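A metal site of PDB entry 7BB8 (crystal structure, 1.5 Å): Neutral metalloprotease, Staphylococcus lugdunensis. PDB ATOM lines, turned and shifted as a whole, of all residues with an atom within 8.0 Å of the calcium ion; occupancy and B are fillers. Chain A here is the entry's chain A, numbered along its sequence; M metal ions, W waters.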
ATOM      1  N   LYS A 103      27.921  20.070   9.779  1.00  0.00           N
ATOM      2  CA  LYS A 103      27.006  21.202   9.736  1.00  0.00           C
ATOM      3  C   LYS A 103      25.813  21.005   8.821  1.00  0.00           C
ATOM      4  O   LYS A 103      24.961  21.908   8.757  1.00  0.00           O
ATOM      5  CB  LYS A 103      27.731  22.473   9.250  1.00  0.00           C
ATOM      6  CG  LYS A 103      28.776  23.021  10.215  1.00  0.00           C
ATOM      7  CD  LYS A 103      28.122  23.550  11.465  1.00  0.00           C
ATOM      8  CE  LYS A 103      28.817  24.779  11.978  1.00  0.00           C
ATOM      9  NZ  LYS A 103      27.986  25.438  13.027  1.00  0.00           N
ATOM     10  N   PRO A 140      23.351  30.386  11.059  1.00  0.00           N
ATOM     11  CA  PRO A 140      21.945  30.005  10.984  1.00  0.00           C
ATOM     12  C   PRO A 140      21.309  29.936  12.352  1.00  0.00           C
ATOM     13  O   PRO A 140      21.957  29.852  13.395  1.00  0.00           O
ATOM     14  CB  PRO A 140      21.990  28.628  10.308  1.00  0.00           C
ATOM     15  CG  PRO A 140      23.285  28.044  10.776  1.00  0.00           C
ATOM     16  CD  PRO A 140      24.243  29.216  10.835  1.00  0.00           C
ATOM     17  N   SER A 141      19.987  30.045  12.328  1.00  0.00           N
ATOM     18  CA  SER A 141      19.169  29.661  13.476  1.00  0.00           C
ATOM     19  C   SER A 141      19.316  28.164  13.743  1.00  0.00           C
ATOM     20  O   SER A 141      19.971  27.439  12.967  1.00  0.00           O
ATOM     21  CB  SER A 141      17.696  30.025  13.209  1.00  0.00           C
ATOM     22  OG  SER A 141      17.212  29.463  12.018  1.00  0.00           O
ATOM     23  N   ASP A 142      18.709  27.683  14.818  1.00  0.00           N
ATOM     24  CA  ASP A 142      18.669  26.224  15.047  1.00  0.00           C
ATOM     25  C   ASP A 142      17.348  25.887  15.751  1.00  0.00           C
ATOM     26  O   ASP A 142      17.298  25.446  16.920  1.00  0.00           O
ATOM     27  CB  ASP A 142      19.868  25.765  15.867  1.00  0.00           C
ATOM     28  CG  ASP A 142      20.068  24.261  15.839  1.00  0.00           C
ATOM     29  OD1 ASP A 142      19.378  23.533  15.074  1.00  0.00           O
ATOM     30  OD2 ASP A 142      20.919  23.824  16.638  1.00  0.00           O
ATOM     31  N   VAL A 143      16.246  26.061  15.022  1.00  0.00           N
ATOM     32  CA  VAL A 143      14.931  25.923  15.627  1.00  0.00           C
ATOM     33  C   VAL A 143      14.640  24.485  16.001  1.00  0.00           C
ATOM     34  O   VAL A 143      13.811  24.250  16.882  1.00  0.00           O
ATOM     35  CB  VAL A 143      13.829  26.453  14.685  1.00  0.00           C
ATOM     36  CG1 VAL A 143      14.119  27.912  14.351  1.00  0.00           C
ATOM     37  CG2 VAL A 143      13.685  25.612  13.409  1.00  0.00           C
ATOM     38  N   ASP A 144      15.306  23.519  15.381  1.00  0.00           N
ATOM     39  CA  ASP A 144      15.118  22.113  15.719  1.00  0.00           C
ATOM     40  C   ASP A 144      16.221  21.589  16.634  1.00  0.00           C
ATOM     41  O   ASP A 144      16.300  20.370  16.845  1.00  0.00           O
ATOM     42  CB  ASP A 144      14.994  21.280  14.453  1.00  0.00           C
ATOM     43  CG  ASP A 144      16.173  21.454  13.485  1.00  0.00           C
ATOM     44  OD1 ASP A 144      17.097  22.237  13.738  1.00  0.00           O
ATOM     45  OD2 ASP A 144      16.142  20.783  12.438  1.00  0.00           O
ATOM     46  N   ASN A 145      17.094  22.470  17.142  1.00  0.00           N
ATOM     47  CA  ASN A 145      18.056  22.117  18.181  1.00  0.00           C
ATOM     48  C   ASN A 145      18.989  20.966  17.796  1.00  0.00           C
ATOM     49  O   ASN A 145      19.293  20.099  18.623  1.00  0.00           O
ATOM     50  CB  ASN A 145      17.302  21.753  19.477  1.00  0.00           C
ATOM     51  CG  ASN A 145      16.332  22.820  19.889  1.00  0.00           C
ATOM     52  OD1 ASN A 145      15.117  22.594  20.012  1.00  0.00           O
ATOM     53  ND2 ASN A 145      16.867  23.997  20.103  1.00  0.00           N
ATOM     54  N   ASN A 146      19.435  20.928  16.557  1.00  0.00           N
ATOM     55  CA  ASN A 146      20.241  19.786  16.122  1.00  0.00           C
ATOM     56  C   ASN A 146      21.625  20.163  15.620  1.00  0.00           C
ATOM     57  O   ASN A 146      22.381  19.267  15.194  1.00  0.00           O
ATOM     58  CB  ASN A 146      19.497  18.976  15.039  1.00  0.00           C
ATOM     59  CG  ASN A 146      19.423  19.688  13.704  1.00  0.00           C
ATOM     60  OD1 ASN A 146      19.758  20.860  13.583  1.00  0.00           O
ATOM     61  ND2 ASN A 146      18.996  18.952  12.668  1.00  0.00           N
ATOM     62  N   GLY A 147      21.983  21.427  15.639  1.00  0.00           N
ATOM     63  CA  GLY A 147      23.312  21.850  15.245  1.00  0.00           C
ATOM     64  C   GLY A 147      23.587  21.830  13.770  1.00  0.00           C
ATOM     65  O   GLY A 147      24.723  22.146  13.375  1.00  0.00           O
ATOM     66  N   LYS A 148      22.615  21.511  12.928  1.00  0.00           N
ATOM     67  CA  LYS A 148      22.884  21.297  11.524  1.00  0.00           C
ATOM     68  C   LYS A 148      21.789  21.929  10.679  1.00  0.00           C
ATOM     69  O   LYS A 148      20.751  22.332  11.196  1.00  0.00           O
ATOM     70  CB  LYS A 148      22.995  19.814  11.196  1.00  0.00           C
ATOM     71  CG  LYS A 148      23.919  19.053  12.115  1.00  0.00           C
ATOM     72  CD  LYS A 148      24.102  17.634  11.677  1.00  0.00           C
ATOM     73  CE  LYS A 148      25.049  16.941  12.631  1.00  0.00           C
ATOM     74  NZ  LYS A 148      25.392  15.610  12.169  1.00  0.00           N
ATOM     75  N   VAL A 149      22.047  22.004   9.380  1.00  0.00           N
ATOM     76  CA  VAL A 149      21.043  22.454   8.423  1.00  0.00           C
ATOM     77  C   VAL A 149      20.757  21.307   7.463  1.00  0.00           C
ATOM     78  O   VAL A 149      21.631  20.471   7.151  1.00  0.00           O
ATOM     79  CB  VAL A 149      21.451  23.717   7.629  1.00  0.00           C
ATOM     80  CG1 VAL A 149      21.931  24.825   8.607  1.00  0.00           C
ATOM     81  CG2 VAL A 149      22.502  23.408   6.656  1.00  0.00           C
ATOM     82  N   ASN A 150      19.534  21.284   6.961  1.00  0.00           N
ATOM     83  CA  ASN A 150      19.123  20.311   5.967  1.00  0.00           C
ATOM     84  C   ASN A 150      19.282  20.874   4.571  1.00  0.00           C
ATOM     85  O   ASN A 150      18.902  22.016   4.314  1.00  0.00           O
ATOM     86  CB  ASN A 150      17.653  19.941   6.153  1.00  0.00           C
ATOM     87  CG  ASN A 150      17.389  19.207   7.429  1.00  0.00           C
ATOM     88  OD1 ASN A 150      18.134  18.292   7.799  1.00  0.00           O
ATOM     89  ND2 ASN A 150      16.329  19.594   8.129  1.00  0.00           N
ATOM     90  N   LEU A 176      11.138  28.232   9.496  1.00  0.00           N
ATOM     91  CA  LEU A 176      11.680  28.555  10.808  1.00  0.00           C
ATOM     92  C   LEU A 176      10.583  28.750  11.867  1.00  0.00           C
ATOM     93  O   LEU A 176      10.909  29.020  13.023  1.00  0.00           O
ATOM     94  CB  LEU A 176      12.563  29.787  10.727  1.00  0.00           C
ATOM     95  CG  LEU A 176      13.711  29.687   9.722  1.00  0.00           C
ATOM     96  CD1 LEU A 176      14.572  30.950   9.740  1.00  0.00           C
ATOM     97  CD2 LEU A 176      14.583  28.479  10.002  1.00  0.00           C
ATOM     98  N   HIS A 184       9.766  23.064   9.960  1.00  0.00           N
ATOM     99  CA  HIS A 184      10.314  23.354  11.266  1.00  0.00           C
ATOM    100  C   HIS A 184      11.788  22.934  11.378  1.00  0.00           C
ATOM    101  O   HIS A 184      12.178  22.097  12.197  1.00  0.00           O
ATOM    102  CB  HIS A 184       9.500  22.700  12.386  1.00  0.00           C
ATOM    103  CG  HIS A 184       9.763  23.328  13.709  1.00  0.00           C
ATOM    104  ND1 HIS A 184      10.551  22.734  14.679  1.00  0.00           N
ATOM    105  CD2 HIS A 184       9.432  24.546  14.178  1.00  0.00           C
ATOM    106  CE1 HIS A 184      10.627  23.547  15.718  1.00  0.00           C
ATOM    107  NE2 HIS A 184       9.973  24.653  15.435  1.00  0.00           N
ATOM    108  N   SER A 185      12.591  23.558  10.534  1.00  0.00           N
ATOM    109  CA  SER A 185      14.021  23.253  10.502  1.00  0.00           C
ATOM    110  C   SER A 185      14.693  24.271   9.622  1.00  0.00           C
ATOM    111  O   SER A 185      14.056  24.950   8.828  1.00  0.00           O
ATOM    112  CB  SER A 185      14.302  21.842   9.959  1.00  0.00           C
ATOM    113  OG  SER A 185      13.872  21.709   8.634  1.00  0.00           O
ATOM    114  N   GLU A 186      15.999  24.411   9.830  1.00  0.00           N
ATOM    115  CA  GLU A 186      16.844  25.055   8.825  1.00  0.00           C
ATOM    116  C   GLU A 186      16.971  24.109   7.648  1.00  0.00           C
ATOM    117  O   GLU A 186      17.526  23.021   7.767  1.00  0.00           O
ATOM    118  CB  GLU A 186      18.201  25.365   9.425  1.00  0.00           C
ATOM    119  CG  GLU A 186      18.171  26.420  10.501  1.00  0.00           C
ATOM    120  CD  GLU A 186      17.507  25.965  11.796  1.00  0.00           C
ATOM    121  OE1 GLU A 186      16.793  26.777  12.429  1.00  0.00           O
ATOM    122  OE2 GLU A 186      17.696  24.787  12.188  1.00  0.00           O
ATOM    123  N   ILE A 187      16.432  24.517   6.517  1.00  0.00           N
ATOM    124  CA  ILE A 187      16.435  23.715   5.308  1.00  0.00           C
ATOM    125  C   ILE A 187      16.524  24.662   4.127  1.00  0.00           C
ATOM    126  O   ILE A 187      15.949  25.759   4.132  1.00  0.00           O
ATOM    127  CB  ILE A 187      15.177  22.824   5.269  1.00  0.00           C
ATOM    128  CG1 ILE A 187      15.181  21.989   4.011  1.00  0.00           C
ATOM    129  CG2 ILE A 187      13.854  23.648   5.379  1.00  0.00           C
ATOM    130  CD1 ILE A 187      14.175  20.842   4.063  1.00  0.00           C
ATOM    131  N   MET A 219      19.594  32.200   4.446  1.00  0.00           N
ATOM    132  CA  MET A 219      19.246  31.593   5.723  1.00  0.00           C
ATOM    133  C   MET A 219      19.849  32.355   6.889  1.00  0.00           C
ATOM    134  O   MET A 219      19.176  32.612   7.879  1.00  0.00           O
ATOM    135  CB  MET A 219      19.698  30.130   5.727  1.00  0.00           C
ATOM    136  CG  MET A 219      19.419  29.412   6.999  1.00  0.00           C
ATOM    137  SD  MET A 219      19.916  27.688   6.882  1.00  0.00           S
ATOM    138  CE  MET A 219      18.585  27.033   5.879  1.00  0.00           C
HETATM  139 CA    CA M   1      19.105  22.992  12.731  1.00  0.00          CA
HETATM  140  O   HOH W   1      20.688  24.883  12.567  1.00  0.00           O
HETATM  141  O   HOH W   2      17.881  21.905  10.792  1.00  0.00           O
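The side-chain carboxylate (OE1) of Glu 186 is in hydrogen-bond range of the side-chain hydroxyl (OG) of Ser 141 (2.7 Å). N of Gly 147 is in hydrogen-bond range of OD2 of Asp 142 (2.8 Å). N of Asn 145 lies close to OD1 of Asp 142 (3.3 Å). The side-chain carboxylate of Glu 186 is in hydrogen-bond range of the backbone NH of Val 143 (2.7 Å). The backbone NH (N) of Asn 150 sits at hydrogen-bond distance from the backbone carbonyl oxygen (O) of Glu 186 (2.8 Å).
Five residues have an atom within 4 Å of the calcium ion: Asp 142, Asp 144, Asn 146, Lys 148 and Glu 186.
The calcium ion is bound by the side-chain carboxylate of Glu 186 (2.3 Å), the backbone carbonyl oxygen of Lys 148 (2.3 Å), the side-chain carboxylate of Asp 144 (2.4 Å), the side-chain amide oxygen of Asn 146 (2.4 Å), the side-chain carboxylate of Asp 142 (2.4 Å), water W1 (2.5 Å) and water W2 (2.5 Å).
Water W2 bridges OD2 of Asp 144 and O of Glu 186.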
